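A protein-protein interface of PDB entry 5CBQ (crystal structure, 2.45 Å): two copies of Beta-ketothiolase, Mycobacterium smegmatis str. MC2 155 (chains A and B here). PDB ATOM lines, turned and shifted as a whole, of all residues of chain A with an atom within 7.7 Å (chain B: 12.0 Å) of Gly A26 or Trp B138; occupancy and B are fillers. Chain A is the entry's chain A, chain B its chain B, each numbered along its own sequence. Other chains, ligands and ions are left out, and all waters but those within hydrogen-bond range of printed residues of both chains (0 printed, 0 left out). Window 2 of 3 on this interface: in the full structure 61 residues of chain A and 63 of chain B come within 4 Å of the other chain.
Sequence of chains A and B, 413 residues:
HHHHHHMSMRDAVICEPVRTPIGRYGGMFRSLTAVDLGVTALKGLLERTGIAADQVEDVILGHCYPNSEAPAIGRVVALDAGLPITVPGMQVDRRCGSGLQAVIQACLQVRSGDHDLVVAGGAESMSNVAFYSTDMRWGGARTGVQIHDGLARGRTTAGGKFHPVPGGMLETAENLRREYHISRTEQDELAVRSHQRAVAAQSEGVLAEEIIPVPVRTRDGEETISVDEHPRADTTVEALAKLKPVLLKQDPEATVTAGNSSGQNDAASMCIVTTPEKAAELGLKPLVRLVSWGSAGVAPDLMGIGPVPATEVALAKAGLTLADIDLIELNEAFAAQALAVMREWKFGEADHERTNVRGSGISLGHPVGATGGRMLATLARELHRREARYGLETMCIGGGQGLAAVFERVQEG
No position is printed for both chains.
Of the 11 pairs that touch across the chains among the printed residues, none has its exchanged pair printed and touching as well.
Among the printed residues, merely in contact across the chains: Tyr A25 with Trp B138 (3.8 Å), Gly A26 with Trp B138 (3.6 Å), Arg A30 with Trp B138 (3.9 Å), Ser A127 with Arg B137 (3.0 Å), Asn A128 with Thr B134 (3.9 Å), Phe A131 with Tyr B132 (3.3 Å) and Phe A131 with Arg B137 (3.5 Å).
The backbone carbonyl oxygen (O) of Arg A30 lies close to the side-chain amide oxygen (OD1) of Asn A128.
The side-chain hydroxyl (OG) of Ser B133 is in hydrogen-bond range of the backbone NH (N) of Asp B135.
The side-chain amide oxygen (OD1) of Asn A128 lies within hydrogen-bond range of the side-chain hydroxyl (OG) of Ser A125 (3.3 Å).
The backbone NH of Tyr A25 sits at hydrogen-bond distance from the backbone carbonyl oxygen of Gln A264 (2.9 Å).
The side-chain hydroxyl (OG) of Ser A127 lies within hydrogen-bond range of the side-chain carboxylate (OD2) of Asp A266.
The side-chain hydroxyl of Ser B133 sits at hydrogen-bond distance from the backbone carbonyl oxygen of Gln B146.
The indole nitrogen of Trp B138 lies within hydrogen-bond range of the backbone carbonyl oxygen of Ser A127, at 2.8 Å.
The side-chain hydroxyl (OH) of Tyr A25 is in hydrogen-bond range of the guanidinium group (NE) of Arg B137, 3.0 Å away.
The guanidinium group (NH1) of Arg B137 lies within hydrogen-bond range of the backbone carbonyl oxygen (O) of Val A129, at 2.5 Å.
The backbone carbonyl oxygen (O) of Phe A131 sits at hydrogen-bond distance from the backbone NH (N) of Ser B133, at 3.0 Å.
Of the 19 printed residues of chain A, 7 touch a printed residue of chain B.
Among the printed residues, 11 pairs touch across the chains.
Of the printed residues of chain B, Tyr A25 touches Arg B137 and Trp B138.
Gly A26 touches one residue of chain B.
No residue of chain B comes within 4 Å of Gly A27.
Of chain B, only Trp B138 (3.9 Å) comes within 4 Å of Arg A30.
Of chain B, only Thr B134 (3.9 Å) comes within 4 Å of Asn A128.
Printed residues of chain B within 4 Å of Phe A131: Tyr B132 (3.3 Å), Ser B133 (3.0 Å) and Arg B137 (3.5 Å).
Gln A264 touches none of the printed residues of chain B.
Printed residues of chain A within 4 Å of Tyr B132: Phe A131 (3.3 Å).
Of the printed residues of chain A, Ser B133 touches Phe A131 (3.0 Å).
Of the printed residues of chain A, Thr B134 touches Asn A128.
Of the printed residues of chain A, Arg B137 touches Tyr A25, Ser A127, Val A129 and Phe A131.
Trp B138 touches four residues of chain A.
No residue of chain A comes within 4 Å of Gly B139.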
ATOM      1  N   GLY A  23      -7.512 -29.136 -35.062  1.00  0.00           N
ATOM      2  CA  GLY A  23      -7.483 -27.796 -34.533  1.00  0.00           C
ATOM      3  C   GLY A  23      -6.521 -26.857 -35.202  1.00  0.00           C
ATOM      4  O   GLY A  23      -5.550 -27.261 -35.759  1.00  0.00           O
ATOM      5  N   ARG A  24      -6.871 -25.588 -35.176  1.00  0.00           N
ATOM      6  CA  ARG A  24      -6.058 -24.509 -35.663  1.00  0.00           C
ATOM      7  C   ARG A  24      -5.036 -24.091 -34.655  1.00  0.00           C
ATOM      8  O   ARG A  24      -5.262 -24.186 -33.499  1.00  0.00           O
ATOM      9  CB  ARG A  24      -6.916 -23.306 -36.000  1.00  0.00           C
ATOM     10  CG  ARG A  24      -7.964 -23.528 -37.055  1.00  0.00           C
ATOM     11  CD  ARG A  24      -8.628 -22.231 -37.410  1.00  0.00           C
ATOM     12  NE  ARG A  24      -7.702 -21.348 -38.085  1.00  0.00           N
ATOM     13  CZ  ARG A  24      -7.832 -20.032 -38.122  1.00  0.00           C
ATOM     14  NH1 ARG A  24      -8.854 -19.472 -37.523  1.00  0.00           N
ATOM     15  NH2 ARG A  24      -6.943 -19.284 -38.756  1.00  0.00           N
ATOM     16  N   TYR A  25      -3.927 -23.561 -35.118  1.00  0.00           N
ATOM     17  CA  TYR A  25      -2.889 -23.115 -34.249  1.00  0.00           C
ATOM     18  C   TYR A  25      -3.468 -22.038 -33.399  1.00  0.00           C
ATOM     19  O   TYR A  25      -4.062 -21.138 -33.888  1.00  0.00           O
ATOM     20  CB  TYR A  25      -1.780 -22.566 -35.125  1.00  0.00           C
ATOM     21  CG  TYR A  25      -0.635 -21.940 -34.405  1.00  0.00           C
ATOM     22  CD1 TYR A  25       0.134 -22.650 -33.523  1.00  0.00           C
ATOM     23  CD2 TYR A  25      -0.305 -20.644 -34.635  1.00  0.00           C
ATOM     24  CE1 TYR A  25       1.186 -22.064 -32.882  1.00  0.00           C
ATOM     25  CE2 TYR A  25       0.743 -20.058 -34.001  1.00  0.00           C
ATOM     26  CZ  TYR A  25       1.475 -20.772 -33.131  1.00  0.00           C
ATOM     27  OH  TYR A  25       2.493 -20.174 -32.522  1.00  0.00           O
ATOM     28  N   GLY A  26      -3.351 -22.193 -32.105  1.00  0.00           N
ATOM     29  CA  GLY A  26      -3.925 -21.283 -31.149  1.00  0.00           C
ATOM     30  C   GLY A  26      -5.403 -21.447 -30.837  1.00  0.00           C
ATOM     31  O   GLY A  26      -5.930 -20.737 -30.032  1.00  0.00           O
ATOM     32  N   GLY A  27      -6.073 -22.378 -31.471  1.00  0.00           N
ATOM     33  CA  GLY A  27      -7.506 -22.503 -31.385  1.00  0.00           C
ATOM     34  C   GLY A  27      -8.004 -23.532 -30.398  1.00  0.00           C
ATOM     35  O   GLY A  27      -7.564 -23.584 -29.280  1.00  0.00           O
ATOM     36  N   MET A  28      -8.820 -24.448 -30.881  1.00  0.00           N
ATOM     37  CA  MET A  28      -9.707 -25.302 -30.116  1.00  0.00           C
ATOM     38  C   MET A  28      -8.959 -26.036 -29.049  1.00  0.00           C
ATOM     39  O   MET A  28      -9.366 -26.088 -27.926  1.00  0.00           O
ATOM     40  CB  MET A  28     -10.061 -26.398 -31.099  1.00  0.00           C
ATOM     41  CG  MET A  28     -11.464 -26.893 -31.208  1.00  0.00           C
ATOM     42  SD  MET A  28     -11.879 -27.296 -32.883  1.00  0.00           S
ATOM     43  CE  MET A  28     -11.143 -28.841 -33.199  1.00  0.00           C
ATOM     44  N   PHE A  29      -7.835 -26.594 -29.432  1.00  0.00           N
ATOM     45  CA  PHE A  29      -7.086 -27.517 -28.618  1.00  0.00           C
ATOM     46  C   PHE A  29      -5.842 -26.926 -28.022  1.00  0.00           C
ATOM     47  O   PHE A  29      -4.969 -27.628 -27.652  1.00  0.00           O
ATOM     48  CB  PHE A  29      -6.723 -28.755 -29.409  1.00  0.00           C
ATOM     49  CG  PHE A  29      -7.886 -29.555 -29.836  1.00  0.00           C
ATOM     50  CD1 PHE A  29      -8.904 -29.786 -28.984  1.00  0.00           C
ATOM     51  CD2 PHE A  29      -7.956 -30.062 -31.084  1.00  0.00           C
ATOM     52  CE1 PHE A  29      -9.970 -30.514 -29.356  1.00  0.00           C
ATOM     53  CE2 PHE A  29      -9.030 -30.811 -31.471  1.00  0.00           C
ATOM     54  CZ  PHE A  29     -10.045 -31.025 -30.599  1.00  0.00           C
ATOM     55  N   ARG A  30      -5.791 -25.622 -27.900  1.00  0.00           N
ATOM     56  CA  ARG A  30      -4.607 -24.953 -27.440  1.00  0.00           C
ATOM     57  C   ARG A  30      -4.236 -25.362 -26.042  1.00  0.00           C
ATOM     58  O   ARG A  30      -3.118 -25.253 -25.657  1.00  0.00           O
ATOM     59  CB  ARG A  30      -4.792 -23.458 -27.520  1.00  0.00           C
ATOM     60  CG  ARG A  30      -3.632 -22.666 -26.977  1.00  0.00           C
ATOM     61  CD  ARG A  30      -3.839 -21.181 -27.148  1.00  0.00           C
ATOM     62  NE  ARG A  30      -5.140 -20.787 -26.648  1.00  0.00           N
ATOM     63  CZ  ARG A  30      -5.331 -20.086 -25.545  1.00  0.00           C
ATOM     64  NH1 ARG A  30      -4.309 -19.686 -24.810  1.00  0.00           N
ATOM     65  NH2 ARG A  30      -6.551 -19.782 -25.174  1.00  0.00           N
ATOM     66  N   SER A  31      -5.186 -25.848 -25.281  1.00  0.00           N
ATOM     67  CA  SER A  31      -4.930 -26.247 -23.924  1.00  0.00           C
ATOM     68  C   SER A  31      -4.541 -27.707 -23.843  1.00  0.00           C
ATOM     69  O   SER A  31      -4.315 -28.228 -22.789  1.00  0.00           O
ATOM     70  CB  SER A  31      -6.152 -25.997 -23.090  1.00  0.00           C
ATOM     71  OG  SER A  31      -7.249 -26.630 -23.675  1.00  0.00           O
ATOM     72  N   SER A 125       0.867 -31.344 -31.535  1.00  0.00           N
ATOM     73  CA  SER A 125       0.364 -30.057 -31.112  1.00  0.00           C
ATOM     74  C   SER A 125       1.343 -28.966 -31.521  1.00  0.00           C
ATOM     75  O   SER A 125       2.253 -28.682 -30.824  1.00  0.00           O
ATOM     76  CB  SER A 125       0.217 -30.039 -29.615  1.00  0.00           C
ATOM     77  OG  SER A 125      -0.569 -28.969 -29.188  1.00  0.00           O
ATOM     78  N   MET A 126       1.117 -28.363 -32.659  1.00  0.00           N
ATOM     79  CA  MET A 126       1.880 -27.216 -33.104  1.00  0.00           C
ATOM     80  C   MET A 126       1.681 -26.004 -32.210  1.00  0.00           C
ATOM     81  O   MET A 126       2.545 -25.224 -32.061  1.00  0.00           O
ATOM     82  CB  MET A 126       1.649 -26.949 -34.576  1.00  0.00           C
ATOM     83  CG  MET A 126       2.092 -28.117 -35.411  1.00  0.00           C
ATOM     84  SD  MET A 126       1.687 -28.206 -37.136  1.00  0.00           S
ATOM     85  CE  MET A 126       2.957 -27.186 -37.816  1.00  0.00           C
ATOM     86  N   SER A 127       0.550 -25.927 -31.554  1.00  0.00           N
ATOM     87  CA  SER A 127       0.262 -24.860 -30.651  1.00  0.00           C
ATOM     88  C   SER A 127       1.206 -24.851 -29.519  1.00  0.00           C
ATOM     89  O   SER A 127       1.438 -23.842 -28.915  1.00  0.00           O
ATOM     90  CB  SER A 127      -1.137 -24.956 -30.128  1.00  0.00           C
ATOM     91  OG  SER A 127      -2.042 -24.660 -31.125  1.00  0.00           O
ATOM     92  N   ASN A 128       1.701 -26.011 -29.186  1.00  0.00           N
ATOM     93  CA  ASN A 128       2.489 -26.146 -28.002  1.00  0.00           C
ATOM     94  C   ASN A 128       3.919 -26.478 -28.181  1.00  0.00           C
ATOM     95  O   ASN A 128       4.578 -26.804 -27.251  1.00  0.00           O
ATOM     96  CB  ASN A 128       1.816 -27.072 -27.049  1.00  0.00           C
ATOM     97  CG  ASN A 128       0.621 -26.456 -26.435  1.00  0.00           C
ATOM     98  OD1 ASN A 128      -0.452 -26.960 -26.531  1.00  0.00           O
ATOM     99  ND2 ASN A 128       0.808 -25.370 -25.802  1.00  0.00           N
ATOM    100  N   VAL A 129       4.403 -26.341 -29.389  1.00  0.00           N
ATOM    101  CA  VAL A 129       5.755 -26.649 -29.703  1.00  0.00           C
ATOM    102  C   VAL A 129       6.637 -25.745 -28.909  1.00  0.00           C
ATOM    103  O   VAL A 129       6.315 -24.619 -28.665  1.00  0.00           O
ATOM    104  CB  VAL A 129       6.019 -26.472 -31.183  1.00  0.00           C
ATOM    105  CG1 VAL A 129       7.470 -26.682 -31.522  1.00  0.00           C
ATOM    106  CG2 VAL A 129       5.173 -27.422 -31.953  1.00  0.00           C
ATOM    107  N   PHE A 131       9.955 -23.593 -27.464  1.00  0.00           N
ATOM    108  CA  PHE A 131      10.962 -22.634 -27.736  1.00  0.00           C
ATOM    109  C   PHE A 131      12.168 -23.250 -27.099  1.00  0.00           C
ATOM    110  O   PHE A 131      12.041 -23.873 -26.115  1.00  0.00           O
ATOM    111  CB  PHE A 131      10.606 -21.290 -27.082  1.00  0.00           C
ATOM    112  CG  PHE A 131       9.865 -20.370 -27.977  1.00  0.00           C
ATOM    113  CD1 PHE A 131       8.533 -20.500 -28.145  1.00  0.00           C
ATOM    114  CD2 PHE A 131      10.516 -19.409 -28.677  1.00  0.00           C
ATOM    115  CE1 PHE A 131       7.859 -19.686 -28.995  1.00  0.00           C
ATOM    116  CE2 PHE A 131       9.853 -18.593 -29.527  1.00  0.00           C
ATOM    117  CZ  PHE A 131       8.517 -18.727 -29.684  1.00  0.00           C
ATOM    118  N   GLU A 229     -11.949 -27.421 -37.079  1.00  0.00           N
ATOM    119  CA  GLU A 229     -12.067 -25.972 -36.918  1.00  0.00           C
ATOM    120  C   GLU A 229     -12.014 -25.174 -38.200  1.00  0.00           C
ATOM    121  O   GLU A 229     -12.789 -24.278 -38.416  1.00  0.00           O
ATOM    122  CB  GLU A 229     -10.965 -25.482 -35.986  1.00  0.00           C
ATOM    123  CG  GLU A 229     -11.193 -24.149 -35.329  1.00  0.00           C
ATOM    124  CD  GLU A 229     -10.284 -23.875 -34.153  1.00  0.00           C
ATOM    125  OE1 GLU A 229      -9.359 -24.619 -33.916  1.00  0.00           O
ATOM    126  OE2 GLU A 229     -10.501 -22.892 -33.446  1.00  0.00           O
ATOM    127  N   GLN A 264      -1.022 -24.447 -39.472  1.00  0.00           N
ATOM    128  CA  GLN A 264      -0.429 -25.202 -38.407  1.00  0.00           C
ATOM    129  C   GLN A 264      -1.486 -25.687 -37.464  1.00  0.00           C
ATOM    130  O   GLN A 264      -2.379 -24.975 -37.163  1.00  0.00           O
ATOM    131  CB  GLN A 264       0.614 -24.364 -37.738  1.00  0.00           C
ATOM    132  CG  GLN A 264       1.596 -23.882 -38.762  1.00  0.00           C
ATOM    133  CD  GLN A 264       2.637 -22.978 -38.215  1.00  0.00           C
ATOM    134  OE1 GLN A 264       3.786 -23.127 -38.526  1.00  0.00           O
ATOM    135  NE2 GLN A 264       2.242 -22.038 -37.406  1.00  0.00           N
ATOM    136  N   ASN A 265      -1.419 -26.936 -37.044  1.00  0.00           N
ATOM    137  CA  ASN A 265      -2.562 -27.600 -36.479  1.00  0.00           C
ATOM    138  C   ASN A 265      -2.303 -28.592 -35.351  1.00  0.00           C
ATOM    139  O   ASN A 265      -1.208 -29.000 -35.118  1.00  0.00           O
ATOM    140  CB  ASN A 265      -3.320 -28.272 -37.608  1.00  0.00           C
ATOM    141  CG  ASN A 265      -3.941 -27.294 -38.579  1.00  0.00           C
ATOM    142  OD1 ASN A 265      -3.510 -27.144 -39.690  1.00  0.00           O
ATOM    143  ND2 ASN A 265      -4.998 -26.692 -38.168  1.00  0.00           N
ATOM    144  N   ASP A 266      -3.360 -28.966 -34.658  1.00  0.00           N
ATOM    145  CA  ASP A 266      -3.336 -29.940 -33.588  1.00  0.00           C
ATOM    146  C   ASP A 266      -4.301 -31.085 -33.779  1.00  0.00           C
ATOM    147  O   ASP A 266      -5.458 -30.888 -33.927  1.00  0.00           O
ATOM    148  CB  ASP A 266      -3.681 -29.268 -32.280  1.00  0.00           C
ATOM    149  CG  ASP A 266      -2.962 -28.000 -32.079  1.00  0.00           C
ATOM    150  OD1 ASP A 266      -1.855 -27.882 -32.552  1.00  0.00           O
ATOM    151  OD2 ASP A 266      -3.501 -27.125 -31.427  1.00  0.00           O
ATOM    152  N   TYR B 132      14.476 -26.025 -22.995  1.00  0.00           N
ATOM    153  CA  TYR B 132      13.220 -25.730 -23.669  1.00  0.00           C
ATOM    154  C   TYR B 132      12.135 -25.213 -22.733  1.00  0.00           C
ATOM    155  O   TYR B 132      12.200 -25.393 -21.558  1.00  0.00           O
ATOM    156  CB  TYR B 132      12.731 -26.938 -24.509  1.00  0.00           C
ATOM    157  CG  TYR B 132      12.170 -28.036 -23.706  1.00  0.00           C
ATOM    158  CD1 TYR B 132      12.976 -28.990 -23.159  1.00  0.00           C
ATOM    159  CD2 TYR B 132      10.860 -28.084 -23.438  1.00  0.00           C
ATOM    160  CE1 TYR B 132      12.480 -29.981 -22.377  1.00  0.00           C
ATOM    161  CE2 TYR B 132      10.354 -29.067 -22.668  1.00  0.00           C
ATOM    162  CZ  TYR B 132      11.170 -30.008 -22.142  1.00  0.00           C
ATOM    163  OH  TYR B 132      10.655 -30.961 -21.375  1.00  0.00           O
ATOM    164  N   SER B 133      11.150 -24.529 -23.290  1.00  0.00           N
ATOM    165  CA  SER B 133       9.998 -24.100 -22.545  1.00  0.00           C
ATOM    166  C   SER B 133       8.749 -24.222 -23.362  1.00  0.00           C
ATOM    167  O   SER B 133       8.761 -24.056 -24.528  1.00  0.00           O
ATOM    168  CB  SER B 133      10.167 -22.671 -22.070  1.00  0.00           C
ATOM    169  OG  SER B 133       9.216 -22.337 -21.135  1.00  0.00           O
ATOM    170  N   THR B 134       7.660 -24.522 -22.704  1.00  0.00           N
ATOM    171  CA  THR B 134       6.369 -24.547 -23.338  1.00  0.00           C
ATOM    172  C   THR B 134       5.495 -23.427 -22.823  1.00  0.00           C
ATOM    173  O   THR B 134       4.305 -23.408 -22.993  1.00  0.00           O
ATOM    174  CB  THR B 134       5.680 -25.916 -23.188  1.00  0.00           C
ATOM    175  OG1 THR B 134       5.608 -26.264 -21.834  1.00  0.00           O
ATOM    176  CG2 THR B 134       6.445 -26.977 -23.874  1.00  0.00           C
ATOM    177  N   ASP B 135       6.122 -22.505 -22.136  1.00  0.00           N
ATOM    178  CA  ASP B 135       5.433 -21.427 -21.523  1.00  0.00           C
ATOM    179  C   ASP B 135       5.621 -20.127 -22.340  1.00  0.00           C
ATOM    180  O   ASP B 135       4.887 -19.186 -22.205  1.00  0.00           O
ATOM    181  CB  ASP B 135       5.960 -21.295 -20.106  1.00  0.00           C
ATOM    182  CG  ASP B 135       5.522 -22.400 -19.205  1.00  0.00           C
ATOM    183  OD1 ASP B 135       4.392 -22.835 -19.290  1.00  0.00           O
ATOM    184  OD2 ASP B 135       6.287 -22.823 -18.353  1.00  0.00           O
ATOM    185  N   MET B 136       6.639 -20.090 -23.171  1.00  0.00           N
ATOM    186  CA  MET B 136       6.960 -18.923 -23.959  1.00  0.00           C
ATOM    187  C   MET B 136       6.006 -18.520 -25.057  1.00  0.00           C
ATOM    188  O   MET B 136       5.898 -17.405 -25.370  1.00  0.00           O
ATOM    189  CB  MET B 136       8.392 -18.970 -24.427  1.00  0.00           C
ATOM    190  CG  MET B 136       9.332 -18.898 -23.258  1.00  0.00           C
ATOM    191  SD  MET B 136      11.044 -19.143 -23.573  1.00  0.00           S
ATOM    192  CE  MET B 136      11.630 -19.450 -21.954  1.00  0.00           C
ATOM    193  N   ARG B 137       5.404 -19.469 -25.710  1.00  0.00           N
ATOM    194  CA  ARG B 137       4.626 -19.229 -26.893  1.00  0.00           C
ATOM    195  C   ARG B 137       3.362 -18.403 -26.729  1.00  0.00           C
ATOM    196  O   ARG B 137       3.081 -17.545 -27.500  1.00  0.00           O
ATOM    197  CB  ARG B 137       4.300 -20.594 -27.450  1.00  0.00           C
ATOM    198  CG  ARG B 137       3.594 -20.612 -28.750  1.00  0.00           C
ATOM    199  CD  ARG B 137       3.727 -21.957 -29.342  1.00  0.00           C
ATOM    200  NE  ARG B 137       4.225 -21.808 -30.666  1.00  0.00           N
ATOM    201  CZ  ARG B 137       5.439 -22.108 -31.022  1.00  0.00           C
ATOM    202  NH1 ARG B 137       6.282 -22.580 -30.154  1.00  0.00           N
ATOM    203  NH2 ARG B 137       5.790 -21.939 -32.246  1.00  0.00           N
ATOM    204  N   TRP B 138       2.598 -18.693 -25.712  1.00  0.00           N
ATOM    205  CA  TRP B 138       1.387 -17.977 -25.416  1.00  0.00           C
ATOM    206  C   TRP B 138       1.543 -17.120 -24.168  1.00  0.00           C
ATOM    207  O   TRP B 138       0.622 -16.492 -23.697  1.00  0.00           O
ATOM    208  CB  TRP B 138       0.224 -18.961 -25.300  1.00  0.00           C
ATOM    209  CG  TRP B 138       0.129 -19.814 -26.458  1.00  0.00           C
ATOM    210  CD1 TRP B 138       0.478 -21.094 -26.539  1.00  0.00           C
ATOM    211  CD2 TRP B 138      -0.309 -19.441 -27.735  1.00  0.00           C
ATOM    212  NE1 TRP B 138       0.270 -21.559 -27.768  1.00  0.00           N
ATOM    213  CE2 TRP B 138      -0.198 -20.549 -28.535  1.00  0.00           C
ATOM    214  CE3 TRP B 138      -0.778 -18.266 -28.281  1.00  0.00           C
ATOM    215  CZ2 TRP B 138      -0.552 -20.537 -29.836  1.00  0.00           C
ATOM    216  CZ3 TRP B 138      -1.126 -18.251 -29.565  1.00  0.00           C
ATOM    217  CH2 TRP B 138      -1.012 -19.368 -30.342  1.00  0.00           C
ATOM    218  N   GLY B 139       2.727 -17.136 -23.623  1.00  0.00           N
ATOM    219  CA  GLY B 139       3.020 -16.296 -22.524  1.00  0.00           C
ATOM    220  C   GLY B 139       2.805 -16.927 -21.204  1.00  0.00           C
ATOM    221  O   GLY B 139       2.038 -17.839 -21.078  1.00  0.00           O
ATOM    222  N   GLY B 140       3.545 -16.426 -20.234  1.00  0.00           N
ATOM    223  CA  GLY B 140       3.605 -16.903 -18.875  1.00  0.00           C
ATOM    224  C   GLY B 140       3.093 -15.893 -17.910  1.00  0.00           C
ATOM    225  O   GLY B 140       3.341 -15.926 -16.744  1.00  0.00           O
ATOM    226  N   ALA B 141       2.308 -15.008 -18.449  1.00  0.00           N
ATOM    227  CA  ALA B 141       1.807 -13.862 -17.742  1.00  0.00           C
ATOM    228  C   ALA B 141       1.023 -14.267 -16.547  1.00  0.00           C
ATOM    229  O   ALA B 141       0.999 -13.554 -15.592  1.00  0.00           O
ATOM    230  CB  ALA B 141       0.936 -13.056 -18.655  1.00  0.00           C
ATOM    231  N   ARG B 142       0.350 -15.406 -16.625  1.00  0.00           N
ATOM    232  CA  ARG B 142      -0.360 -15.948 -15.495  1.00  0.00           C
ATOM    233  C   ARG B 142       0.345 -17.068 -14.789  1.00  0.00           C
ATOM    234  O   ARG B 142       0.219 -17.192 -13.627  1.00  0.00           O
ATOM    235  CB  ARG B 142      -1.744 -16.411 -15.922  1.00  0.00           C
ATOM    236  N   THR B 143       0.987 -17.953 -15.525  1.00  0.00           N
ATOM    237  CA  THR B 143       1.506 -19.206 -14.993  1.00  0.00           C
ATOM    238  C   THR B 143       2.913 -19.212 -14.437  1.00  0.00           C
ATOM    239  O   THR B 143       3.280 -20.000 -13.601  1.00  0.00           O
ATOM    240  CB  THR B 143       1.398 -20.289 -16.054  1.00  0.00           C
ATOM    241  OG1 THR B 143       2.164 -19.931 -17.200  1.00  0.00           O
ATOM    242  CG2 THR B 143       0.015 -20.385 -16.463  1.00  0.00           C
ATOM    243  N   GLY B 144       3.709 -18.322 -14.945  1.00  0.00           N
ATOM    244  CA  GLY B 144       5.116 -18.396 -14.802  1.00  0.00           C
ATOM    245  C   GLY B 144       5.758 -19.084 -15.976  1.00  0.00           C
ATOM    246  O   GLY B 144       5.101 -19.514 -16.892  1.00  0.00           O
ATOM    247  N   VAL B 145       7.078 -19.106 -15.962  1.00  0.00           N
ATOM    248  CA  VAL B 145       7.864 -19.746 -16.977  1.00  0.00           C
ATOM    249  C   VAL B 145       8.858 -20.731 -16.402  1.00  0.00           C
ATOM    250  O   VAL B 145       9.633 -20.419 -15.550  1.00  0.00           O
ATOM    251  CB  VAL B 145       8.529 -18.715 -17.880  1.00  0.00           C
ATOM    252  CG1 VAL B 145       9.374 -19.383 -18.937  1.00  0.00           C
ATOM    253  CG2 VAL B 145       7.480 -17.828 -18.507  1.00  0.00           C
ATOM    254  N   GLN B 146       8.827 -21.935 -16.920  1.00  0.00           N
ATOM    255  CA  GLN B 146       9.833 -22.894 -16.607  1.00  0.00           C
ATOM    256  C   GLN B 146      10.586 -23.086 -17.849  1.00  0.00           C
ATOM    257  O   GLN B 146      10.054 -22.943 -18.909  1.00  0.00           O
ATOM    258  CB  GLN B 146       9.224 -24.198 -16.210  1.00  0.00           C
ATOM    259  CG  GLN B 146       8.538 -24.156 -14.894  1.00  0.00           C
ATOM    260  CD  GLN B 146       8.311 -25.514 -14.332  1.00  0.00           C
ATOM    261  OE1 GLN B 146       7.214 -25.980 -14.295  1.00  0.00           O
ATOM    262  NE2 GLN B 146       9.358 -26.143 -13.890  1.00  0.00           N
